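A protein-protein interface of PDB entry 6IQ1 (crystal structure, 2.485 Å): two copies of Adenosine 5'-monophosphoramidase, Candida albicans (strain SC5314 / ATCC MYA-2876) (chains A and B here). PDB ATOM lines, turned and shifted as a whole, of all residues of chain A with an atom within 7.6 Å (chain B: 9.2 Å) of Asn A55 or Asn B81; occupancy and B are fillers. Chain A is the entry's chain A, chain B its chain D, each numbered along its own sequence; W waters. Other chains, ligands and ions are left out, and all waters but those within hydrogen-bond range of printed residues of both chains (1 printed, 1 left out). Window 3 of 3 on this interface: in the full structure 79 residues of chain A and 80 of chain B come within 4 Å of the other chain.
Among the printed residues, pairs that only touch across the chains: Leu A53 with Tyr B88, His A54 with Thr B72, Leu A61 with Lys B69, His A54 with Asn B80, His A54 with Lys B69, His A54 with Leu B77, Asp A103 with Pro B83, Lys A52 with Glu B86 and Pro A57 with Lys B69.
Water W1 lies within hydrogen-bond range of the side-chain amino group (NZ) of Lys A52 (2.8 Å), the backbone carbonyl oxygen (O) of Leu B77 (3.0 Å) and the backbone carbonyl oxygen (O) of Glu B86 (3.4 Å).
His A49 touches none of the printed residues of chain B.
Gly A50 touches none of the printed residues of chain B.
No residue of chain B comes within 4 Å of Ala A51.
Asn A55 touches just one residue of chain B: Asn B81 (3.0 Å).
Ile A56 touches just one residue of chain B: Lys B69 (2.8 Å).
Gln A100 touches none of the printed residues of chain B.
Printed residues of chain A within 4 Å of Lys B69: His A54, Ile A56, Pro A57, Asp A58 and Leu A61.
Printed residues of chain A within 4 Å of Thr B72: His A54.
Printed residues of chain A within 4 Å of Leu B77: His A54.
Of the printed residues of chain A, Asp B78 touches His A54.
Of the printed residues of chain A, Tyr B88 touches Leu A53, His A54 and Asn A94.
The nearest residue of chain A that does not touch Asn B81 is Lys A52 (5.0 Å).
The nearest printed residue of chain A that does not touch Asp B78 is Asn A55 (5.9 Å).
The side-chain amino group (NZ) of Lys A52 sits at hydrogen-bond distance from the backbone carbonyl oxygen (O) of Asn B80 (3.1 Å).
A ring nitrogen (NE2) of His A54 is in hydrogen-bond range of the side-chain amide oxygen (OD1) of Asn B81, at 2.7 Å.
The side-chain amino group (NZ) of Lys B69 lies within salt-bridge range of the side-chain carboxylate (OD1) of Asp A58 (3.2 Å).
The backbone carbonyl oxygen (O) of Tyr B88 sits at hydrogen-bond distance from the backbone NH (N) of Asn A94.
The side-chain amide nitrogen of Asn A55 lies within hydrogen-bond range of the side-chain amide oxygen of Asn B81 (3.0 Å).
O of Thr B82 lies close to NZ of Lys A52.
NE2 of His A54 sits at hydrogen-bond distance from O of Asp B78 (3.4 Å).
OH of Tyr B88 sits at hydrogen-bond distance from ND1 of His A54, 2.8 Å away.
The backbone carbonyl oxygen (O) of Ile A56 lies within hydrogen-bond range of the side-chain amino group (NZ) of Lys B69, at 2.8 Å.
Of the 16 printed residues of chain A, 10 touch a printed residue of chain B.
Printed residues of chain B that touch a printed residue of chain A: Lys B69, Thr B72, Leu B77, Asp B78, Asn B80, Asn B81, Thr B82, Pro B83, Glu B86 and Tyr B88.
Hydrophobic or aromatic side chains of chain B that line the printed part of chain A: Pro B83 and Tyr B88.
Among the printed residues, Asp or Glu carboxylates within 4 Å of a Lys or Arg side-chain nitrogen of the other chain: Asp A58 with Lys B69.
The side-chain hydroxyl (OG1) of Thr B82 is in hydrogen-bond range of the backbone carbonyl oxygen (O) of Glu B84, 3.3 Å away.
ND2 of Asn B80 is in hydrogen-bond range of O of Glu B84, at 2.8 Å.
The side-chain amide nitrogen (ND2) of Asn B80 sits at hydrogen-bond distance from the backbone carbonyl oxygen (O) of Glu B86, at 2.8 Å.
The backbone NH (N) of Lys A52 is in hydrogen-bond range of the side-chain amide oxygen (OD1) of Asn A55 (2.7 Å).
N of Asp B78 is in hydrogen-bond range of O of Thr B72 (3.2 Å).
The backbone NH (N) of Leu A53 lies within hydrogen-bond range of the side-chain amide oxygen (OD1) of Asn A94 (2.9 Å).
No position is printed for both chains.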
ATOM      1  N   HIS A  48       6.643  -5.202  -7.010  1.00  0.00           N
ATOM      2  CA  HIS A  48       7.396  -6.313  -7.568  1.00  0.00           C
ATOM      3  C   HIS A  48       7.181  -7.539  -6.697  1.00  0.00           C
ATOM      4  O   HIS A  48       7.571  -7.541  -5.519  1.00  0.00           O
ATOM      5  CB  HIS A  48       8.881  -5.959  -7.635  1.00  0.00           C
ATOM      6  CG  HIS A  48       9.742  -7.044  -8.199  1.00  0.00           C
ATOM      7  ND1 HIS A  48      10.115  -8.156  -7.472  1.00  0.00           N
ATOM      8  CD2 HIS A  48      10.321  -7.175  -9.416  1.00  0.00           C
ATOM      9  CE1 HIS A  48      10.881  -8.929  -8.223  1.00  0.00           C
ATOM     10  NE2 HIS A  48      11.020  -8.358  -9.406  1.00  0.00           N
ATOM     11  N   HIS A  49       6.577  -8.577  -7.278  1.00  0.00           N
ATOM     12  CA  HIS A  49       6.326  -9.817  -6.559  1.00  0.00           C
ATOM     13  C   HIS A  49       7.635 -10.568  -6.306  1.00  0.00           C
ATOM     14  O   HIS A  49       8.323 -10.977  -7.249  1.00  0.00           O
ATOM     15  CB  HIS A  49       5.349 -10.704  -7.335  1.00  0.00           C
ATOM     16  CG  HIS A  49       5.262 -12.096  -6.798  1.00  0.00           C
ATOM     17  ND1 HIS A  49       4.332 -12.471  -5.854  1.00  0.00           N
ATOM     18  CD2 HIS A  49       6.026 -13.190  -7.028  1.00  0.00           C
ATOM     19  CE1 HIS A  49       4.511 -13.741  -5.542  1.00  0.00           C
ATOM     20  NE2 HIS A  49       5.530 -14.203  -6.245  1.00  0.00           N
ATOM     21  N   GLY A  50       7.974 -10.743  -5.031  1.00  0.00           N
ATOM     22  CA  GLY A  50       9.046 -11.621  -4.609  1.00  0.00           C
ATOM     23  C   GLY A  50       8.682 -12.167  -3.249  1.00  0.00           C
ATOM     24  O   GLY A  50       8.114 -11.427  -2.442  1.00  0.00           O
ATOM     25  N   ALA A  51       8.981 -13.438  -2.968  1.00  0.00           N
ATOM     26  CA  ALA A  51       8.494 -14.045  -1.725  1.00  0.00           C
ATOM     27  C   ALA A  51       9.244 -13.526  -0.505  1.00  0.00           C
ATOM     28  O   ALA A  51       8.637 -13.239   0.529  1.00  0.00           O
ATOM     29  CB  ALA A  51       8.601 -15.567  -1.796  1.00  0.00           C
ATOM     30  N   LYS A  52      10.554 -13.394  -0.595  1.00  0.00           N
ATOM     31  CA  LYS A  52      11.346 -13.003   0.550  1.00  0.00           C
ATOM     32  C   LYS A  52      12.066 -11.694   0.250  1.00  0.00           C
ATOM     33  O   LYS A  52      12.073 -11.216  -0.891  1.00  0.00           O
ATOM     34  CB  LYS A  52      12.336 -14.108   0.912  1.00  0.00           C
ATOM     35  CG  LYS A  52      11.689 -15.354   1.423  1.00  0.00           C
ATOM     36  CD  LYS A  52      12.756 -16.406   1.661  1.00  0.00           C
ATOM     37  CE  LYS A  52      12.209 -17.602   2.380  1.00  0.00           C
ATOM     38  NZ  LYS A  52      13.328 -18.289   3.082  1.00  0.00           N
ATOM     39  N   LEU A  53      12.667 -11.117   1.304  1.00  0.00           N
ATOM     40  CA  LEU A  53      13.306  -9.813   1.188  1.00  0.00           C
ATOM     41  C   LEU A  53      14.396  -9.827   0.125  1.00  0.00           C
ATOM     42  O   LEU A  53      14.503  -8.898  -0.690  1.00  0.00           O
ATOM     43  CB  LEU A  53      13.890  -9.383   2.536  1.00  0.00           C
ATOM     44  CG  LEU A  53      14.371  -7.924   2.540  1.00  0.00           C
ATOM     45  CD1 LEU A  53      13.184  -6.984   2.798  1.00  0.00           C
ATOM     46  CD2 LEU A  53      15.505  -7.687   3.541  1.00  0.00           C
ATOM     47  N   HIS A  54      15.210 -10.873   0.114  1.00  0.00           N
ATOM     48  CA  HIS A  54      16.289 -10.936  -0.849  1.00  0.00           C
ATOM     49  C   HIS A  54      15.790 -11.150  -2.281  1.00  0.00           C
ATOM     50  O   HIS A  54      16.611 -11.126  -3.200  1.00  0.00           O
ATOM     51  CB  HIS A  54      17.267 -12.042  -0.442  1.00  0.00           C
ATOM     52  CG  HIS A  54      16.667 -13.414  -0.455  1.00  0.00           C
ATOM     53  ND1 HIS A  54      16.090 -13.986   0.656  1.00  0.00           N
ATOM     54  CD2 HIS A  54      16.538 -14.321  -1.454  1.00  0.00           C
ATOM     55  CE1 HIS A  54      15.642 -15.190   0.347  1.00  0.00           C
ATOM     56  NE2 HIS A  54      15.898 -15.416  -0.931  1.00  0.00           N
ATOM     57  N   ASN A  55      14.491 -11.372  -2.499  1.00  0.00           N
ATOM     58  CA  ASN A  55      13.946 -11.437  -3.850  1.00  0.00           C
ATOM     59  C   ASN A  55      13.505 -10.074  -4.377  1.00  0.00           C
ATOM     60  O   ASN A  55      13.003  -9.999  -5.495  1.00  0.00           O
ATOM     61  CB  ASN A  55      12.739 -12.388  -3.930  1.00  0.00           C
ATOM     62  CG  ASN A  55      13.012 -13.781  -3.375  1.00  0.00           C
ATOM     63  OD1 ASN A  55      12.299 -14.243  -2.475  1.00  0.00           O
ATOM     64  ND2 ASN A  55      14.003 -14.472  -3.928  1.00  0.00           N
ATOM     65  N   ILE A  56      13.639  -9.000  -3.614  1.00  0.00           N
ATOM     66  CA  ILE A  56      13.158  -7.684  -4.031  1.00  0.00           C
ATOM     67  C   ILE A  56      14.325  -6.865  -4.576  1.00  0.00           C
ATOM     68  O   ILE A  56      15.373  -6.779  -3.916  1.00  0.00           O
ATOM     69  CB  ILE A  56      12.465  -6.928  -2.888  1.00  0.00           C
ATOM     70  CG1 ILE A  56      11.421  -7.800  -2.207  1.00  0.00           C
ATOM     71  CG2 ILE A  56      11.788  -5.694  -3.452  1.00  0.00           C
ATOM     72  CD1 ILE A  56      10.211  -8.069  -3.084  1.00  0.00           C
ATOM     73  N   PRO A  57      14.182  -6.245  -5.744  1.00  0.00           N
ATOM     74  CA  PRO A  57      15.239  -5.355  -6.241  1.00  0.00           C
ATOM     75  C   PRO A  57      15.457  -4.169  -5.302  1.00  0.00           C
ATOM     76  O   PRO A  57      14.553  -3.748  -4.576  1.00  0.00           O
ATOM     77  CB  PRO A  57      14.711  -4.907  -7.609  1.00  0.00           C
ATOM     78  CG  PRO A  57      13.680  -5.965  -7.985  1.00  0.00           C
ATOM     79  CD  PRO A  57      13.066  -6.413  -6.696  1.00  0.00           C
ATOM     80  N   ASP A  58      16.679  -3.621  -5.339  1.00  0.00           N
ATOM     81  CA  ASP A  58      17.041  -2.522  -4.446  1.00  0.00           C
ATOM     82  C   ASP A  58      16.153  -1.302  -4.646  1.00  0.00           C
ATOM     83  O   ASP A  58      15.752  -0.657  -3.668  1.00  0.00           O
ATOM     84  CB  ASP A  58      18.504  -2.132  -4.645  1.00  0.00           C
ATOM     85  CG  ASP A  58      19.453  -3.178  -4.113  1.00  0.00           C
ATOM     86  OD1 ASP A  58      19.006  -4.012  -3.298  1.00  0.00           O
ATOM     87  OD2 ASP A  58      20.632  -3.184  -4.535  1.00  0.00           O
ATOM     88  N   LEU A  61      13.245  -1.728  -2.682  1.00  0.00           N
ATOM     89  CA  LEU A  61      13.505  -1.755  -1.249  1.00  0.00           C
ATOM     90  C   LEU A  61      13.716  -0.357  -0.691  1.00  0.00           C
ATOM     91  O   LEU A  61      13.327  -0.080   0.447  1.00  0.00           O
ATOM     92  CB  LEU A  61      14.713  -2.637  -0.946  1.00  0.00           C
ATOM     93  CG  LEU A  61      14.446  -4.140  -1.033  1.00  0.00           C
ATOM     94  CD1 LEU A  61      15.643  -4.879  -0.505  1.00  0.00           C
ATOM     95  CD2 LEU A  61      13.169  -4.556  -0.272  1.00  0.00           C
ATOM     96  N   ASN A  94      10.003 -13.862   6.725  1.00  0.00           N
ATOM     97  CA  ASN A  94      10.584 -14.586   5.598  1.00  0.00           C
ATOM     98  C   ASN A  94      10.578 -16.070   5.958  1.00  0.00           C
ATOM     99  O   ASN A  94      11.428 -16.538   6.725  1.00  0.00           O
ATOM    100  CB  ASN A  94      11.994 -14.079   5.284  1.00  0.00           C
ATOM    101  CG  ASN A  94      12.021 -12.589   4.972  1.00  0.00           C
ATOM    102  OD1 ASN A  94      11.832 -12.185   3.827  1.00  0.00           O
ATOM    103  ND2 ASN A  94      12.259 -11.765   5.992  1.00  0.00           N
ATOM    104  N   GLN A 100       5.641 -16.104   8.195  1.00  0.00           N
ATOM    105  CA  GLN A 100       5.131 -15.604   6.928  1.00  0.00           C
ATOM    106  C   GLN A 100       4.170 -16.621   6.315  1.00  0.00           C
ATOM    107  O   GLN A 100       4.489 -17.807   6.207  1.00  0.00           O
ATOM    108  CB  GLN A 100       6.284 -15.320   5.962  1.00  0.00           C
ATOM    109  CG  GLN A 100       5.816 -14.830   4.635  1.00  0.00           C
ATOM    110  CD  GLN A 100       6.917 -14.779   3.618  1.00  0.00           C
ATOM    111  OE1 GLN A 100       7.916 -15.481   3.745  1.00  0.00           O
ATOM    112  NE2 GLN A 100       6.736 -13.954   2.577  1.00  0.00           N
ATOM    113  N   ASP A 103       3.159 -15.391   0.453  1.00  0.00           N
ATOM    114  CA  ASP A 103       4.518 -15.492  -0.084  1.00  0.00           C
ATOM    115  C   ASP A 103       4.860 -14.346  -1.033  1.00  0.00           C
ATOM    116  O   ASP A 103       5.294 -14.530  -2.175  1.00  0.00           O
ATOM    117  CB  ASP A 103       4.695 -16.855  -0.743  1.00  0.00           C
ATOM    118  CG  ASP A 103       4.818 -17.973   0.299  1.00  0.00           C
ATOM    119  OD1 ASP A 103       5.407 -17.697   1.376  1.00  0.00           O
ATOM    120  OD2 ASP A 103       4.316 -19.101   0.063  1.00  0.00           O
ATOM    121  N   VAL A 105       6.524 -10.260  -0.298  1.00  0.00           N
ATOM    122  CA  VAL A 105       7.117  -9.506   0.795  1.00  0.00           C
ATOM    123  C   VAL A 105       6.113  -8.491   1.300  1.00  0.00           C
ATOM    124  O   VAL A 105       5.501  -7.772   0.508  1.00  0.00           O
ATOM    125  CB  VAL A 105       8.418  -8.828   0.332  1.00  0.00           C
ATOM    126  CG1 VAL A 105       8.793  -7.660   1.258  1.00  0.00           C
ATOM    127  CG2 VAL A 105       9.511  -9.837   0.286  1.00  0.00           C
ATOM    128  N   LYS B  69      19.347  -6.422   2.739  1.00  0.00           N
ATOM    129  CA  LYS B  69      19.351  -7.408   1.666  1.00  0.00           C
ATOM    130  C   LYS B  69      20.758  -7.926   1.406  1.00  0.00           C
ATOM    131  O   LYS B  69      20.973  -9.137   1.286  1.00  0.00           O
ATOM    132  CB  LYS B  69      18.771  -6.806   0.392  1.00  0.00           C
ATOM    133  CG  LYS B  69      18.919  -7.710  -0.792  1.00  0.00           C
ATOM    134  CD  LYS B  69      18.144  -7.156  -1.953  1.00  0.00           C
ATOM    135  CE  LYS B  69      18.489  -7.864  -3.225  1.00  0.00           C
ATOM    136  NZ  LYS B  69      18.117  -6.942  -4.303  1.00  0.00           N
ATOM    137  N   THR B  72      21.747 -10.435   4.023  1.00  0.00           N
ATOM    138  CA  THR B  72      21.232 -11.790   3.825  1.00  0.00           C
ATOM    139  C   THR B  72      22.110 -12.582   2.853  1.00  0.00           C
ATOM    140  O   THR B  72      22.138 -13.813   2.909  1.00  0.00           O
ATOM    141  CB  THR B  72      19.766 -11.787   3.336  1.00  0.00           C
ATOM    142  OG1 THR B  72      19.658 -11.181   2.039  1.00  0.00           O
ATOM    143  CG2 THR B  72      18.846 -11.066   4.312  1.00  0.00           C
ATOM    144  N   LYS B  73      22.848 -11.904   1.971  1.00  0.00           N
ATOM    145  CA  LYS B  73      23.830 -12.621   1.157  1.00  0.00           C
ATOM    146  C   LYS B  73      25.056 -13.014   1.977  1.00  0.00           C
ATOM    147  O   LYS B  73      25.558 -14.135   1.841  1.00  0.00           O
ATOM    148  CB  LYS B  73      24.250 -11.786  -0.049  1.00  0.00           C
ATOM    149  CG  LYS B  73      23.173 -11.628  -1.117  1.00  0.00           C
ATOM    150  CD  LYS B  73      23.668 -10.721  -2.230  1.00  0.00           C
ATOM    151  CE  LYS B  73      22.511 -10.026  -2.929  1.00  0.00           C
ATOM    152  NZ  LYS B  73      22.911  -9.516  -4.260  1.00  0.00           N
ATOM    153  N   LYS B  76      24.158 -15.956   3.964  1.00  0.00           N
ATOM    154  CA  LYS B  76      23.740 -17.067   3.105  1.00  0.00           C
ATOM    155  C   LYS B  76      22.249 -17.373   3.197  1.00  0.00           C
ATOM    156  O   LYS B  76      21.790 -18.360   2.592  1.00  0.00           O
ATOM    157  CB  LYS B  76      24.541 -18.346   3.389  1.00  0.00           C
ATOM    158  CG  LYS B  76      25.950 -18.388   2.763  1.00  0.00           C
ATOM    159  CD  LYS B  76      26.644 -19.717   3.083  1.00  0.00           C
ATOM    160  CE  LYS B  76      27.497 -20.213   1.922  1.00  0.00           C
ATOM    161  NZ  LYS B  76      28.897 -19.699   1.998  1.00  0.00           N
ATOM    162  N   LEU B  77      21.480 -16.557   3.934  1.00  0.00           N
ATOM    163  CA  LEU B  77      20.025 -16.672   3.951  1.00  0.00           C
ATOM    164  C   LEU B  77      19.408 -16.547   2.560  1.00  0.00           C
ATOM    165  O   LEU B  77      18.274 -16.996   2.355  1.00  0.00           O
ATOM    166  CB  LEU B  77      19.422 -15.593   4.848  1.00  0.00           C
ATOM    167  CG  LEU B  77      19.744 -15.605   6.349  1.00  0.00           C
ATOM    168  CD1 LEU B  77      19.293 -14.319   7.043  1.00  0.00           C
ATOM    169  CD2 LEU B  77      19.094 -16.808   6.996  1.00  0.00           C
ATOM    170  N   ASP B  78      20.109 -15.938   1.600  1.00  0.00           N
ATOM    171  CA  ASP B  78      19.487 -15.743   0.296  1.00  0.00           C
ATOM    172  C   ASP B  78      19.427 -17.026  -0.513  1.00  0.00           C
ATOM    173  O   ASP B  78      18.848 -17.018  -1.604  1.00  0.00           O
ATOM    174  CB  ASP B  78      20.214 -14.651  -0.504  1.00  0.00           C
ATOM    175  CG  ASP B  78      21.592 -15.070  -0.971  1.00  0.00           C
ATOM    176  OD1 ASP B  78      22.303 -15.782  -0.238  1.00  0.00           O
ATOM    177  OD2 ASP B  78      21.976 -14.674  -2.088  1.00  0.00           O
ATOM    178  N   GLU B  79      19.992 -18.119  -0.003  1.00  0.00           N
ATOM    179  CA  GLU B  79      20.083 -19.357  -0.761  1.00  0.00           C
ATOM    180  C   GLU B  79      18.821 -20.200  -0.653  1.00  0.00           C
ATOM    181  O   GLU B  79      18.634 -21.112  -1.464  1.00  0.00           O
ATOM    182  CB  GLU B  79      21.315 -20.154  -0.301  1.00  0.00           C
ATOM    183  CG  GLU B  79      22.638 -19.393  -0.541  1.00  0.00           C
ATOM    184  CD  GLU B  79      23.897 -20.250  -0.408  1.00  0.00           C
ATOM    185  OE1 GLU B  79      23.795 -21.457  -0.101  1.00  0.00           O
ATOM    186  OE2 GLU B  79      25.001 -19.701  -0.613  1.00  0.00           O
ATOM    187  N   ASN B  80      17.942 -19.895   0.303  1.00  0.00           N
ATOM    188  CA  ASN B  80      16.688 -20.615   0.486  1.00  0.00           C
ATOM    189  C   ASN B  80      15.555 -19.785  -0.117  1.00  0.00           C
ATOM    190  O   ASN B  80      15.007 -18.887   0.528  1.00  0.00           O
ATOM    191  CB  ASN B  80      16.445 -20.914   1.958  1.00  0.00           C
ATOM    192  CG  ASN B  80      15.114 -21.591   2.195  1.00  0.00           C
ATOM    193  OD1 ASN B  80      14.510 -22.147   1.271  1.00  0.00           O
ATOM    194  ND2 ASN B  80      14.640 -21.544   3.435  1.00  0.00           N
ATOM    195  N   ASN B  81      15.193 -20.102  -1.355  1.00  0.00           N
ATOM    196  CA  ASN B  81      14.089 -19.436  -2.036  1.00  0.00           C
ATOM    197  C   ASN B  81      12.807 -20.247  -1.941  1.00  0.00           C
ATOM    198  O   ASN B  81      12.010 -20.287  -2.873  1.00  0.00           O
ATOM    199  CB  ASN B  81      14.461 -19.148  -3.489  1.00  0.00           C
ATOM    200  CG  ASN B  81      15.533 -18.067  -3.596  1.00  0.00           C
ATOM    201  OD1 ASN B  81      15.394 -16.972  -3.030  1.00  0.00           O
ATOM    202  ND2 ASN B  81      16.623 -18.381  -4.291  1.00  0.00           N
ATOM    203  N   THR B  82      12.584 -20.907  -0.818  1.00  0.00           N
ATOM    204  CA  THR B  82      11.340 -21.614  -0.566  1.00  0.00           C
ATOM    205  C   THR B  82      10.793 -21.169   0.778  1.00  0.00           C
ATOM    206  O   THR B  82      11.542 -20.660   1.623  1.00  0.00           O
ATOM    207  CB  THR B  82      11.531 -23.146  -0.583  1.00  0.00           C
ATOM    208  OG1 THR B  82      12.097 -23.597   0.657  1.00  0.00           O
ATOM    209  CG2 THR B  82      12.435 -23.569  -1.733  1.00  0.00           C
ATOM    210  N   PRO B  83       9.481 -21.298   0.989  1.00  0.00           N
ATOM    211  CA  PRO B  83       8.916 -20.943   2.300  1.00  0.00           C
ATOM    212  C   PRO B  83       9.228 -21.940   3.398  1.00  0.00           C
ATOM    213  O   PRO B  83       8.946 -21.641   4.561  1.00  0.00           O
ATOM    214  CB  PRO B  83       7.402 -20.869   2.038  1.00  0.00           C
ATOM    215  CG  PRO B  83       7.186 -21.536   0.736  1.00  0.00           C
ATOM    216  CD  PRO B  83       8.446 -21.427  -0.049  1.00  0.00           C
ATOM    217  N   GLU B  84       9.794 -23.099   3.077  1.00  0.00           N
ATOM    218  CA  GLU B  84      10.144 -24.084   4.094  1.00  0.00           C
ATOM    219  C   GLU B  84      11.595 -23.909   4.528  1.00  0.00           C
ATOM    220  O   GLU B  84      12.352 -23.118   3.952  1.00  0.00           O
ATOM    221  CB  GLU B  84       9.913 -25.505   3.582  1.00  0.00           C
ATOM    222  CG  GLU B  84       8.744 -25.647   2.589  1.00  0.00           C
ATOM    223  CD  GLU B  84       7.381 -25.367   3.235  1.00  0.00           C
ATOM    224  OE1 GLU B  84       7.199 -25.648   4.458  1.00  0.00           O
ATOM    225  OE2 GLU B  84       6.496 -24.839   2.507  1.00  0.00           O
ATOM    226  N   GLY B  85      11.996 -24.684   5.531  1.00  0.00           N
ATOM    227  CA  GLY B  85      13.369 -24.612   5.982  1.00  0.00           C
ATOM    228  C   GLY B  85      13.557 -23.404   6.876  1.00  0.00           C
ATOM    229  O   GLY B  85      12.618 -22.917   7.505  1.00  0.00           O
ATOM    230  N   GLU B  86      14.780 -22.907   6.933  1.00  0.00           N
ATOM    231  CA  GLU B  86      15.005 -21.838   7.882  1.00  0.00           C
ATOM    232  C   GLU B  86      14.639 -20.503   7.218  1.00  0.00           C
ATOM    233  O   GLU B  86      14.639 -20.368   5.987  1.00  0.00           O
ATOM    234  CB  GLU B  86      16.445 -21.914   8.379  1.00  0.00           C
ATOM    235  CG  GLU B  86      16.993 -20.701   8.976  1.00  0.00           C
ATOM    236  CD  GLU B  86      18.484 -20.561   8.621  1.00  0.00           C
ATOM    237  OE1 GLU B  86      18.894 -20.631   7.437  1.00  0.00           O
ATOM    238  OE2 GLU B  86      19.224 -20.237   9.505  1.00  0.00           O
ATOM    239  N   TYR B  88      13.881 -15.934   8.413  1.00  0.00           N
ATOM    240  CA  TYR B  88      14.439 -14.783   9.116  1.00  0.00           C
ATOM    241  C   TYR B  88      13.393 -13.680   9.256  1.00  0.00           C
ATOM    242  O   TYR B  88      12.402 -13.623   8.514  1.00  0.00           O
ATOM    243  CB  TYR B  88      15.711 -14.242   8.430  1.00  0.00           C
ATOM    244  CG  TYR B  88      15.599 -13.791   6.982  1.00  0.00           C
ATOM    245  CD1 TYR B  88      15.756 -14.697   5.936  1.00  0.00           C
ATOM    246  CD2 TYR B  88      15.398 -12.452   6.664  1.00  0.00           C
ATOM    247  CE1 TYR B  88      15.680 -14.291   4.613  1.00  0.00           C
ATOM    248  CE2 TYR B  88      15.342 -12.026   5.343  1.00  0.00           C
ATOM    249  CZ  TYR B  88      15.479 -12.950   4.319  1.00  0.00           C
ATOM    250  OH  TYR B  88      15.395 -12.536   3.005  1.00  0.00           O
HETATM  251  O   HOH W   1      15.952 -17.905   3.975  1.00  0.00           O
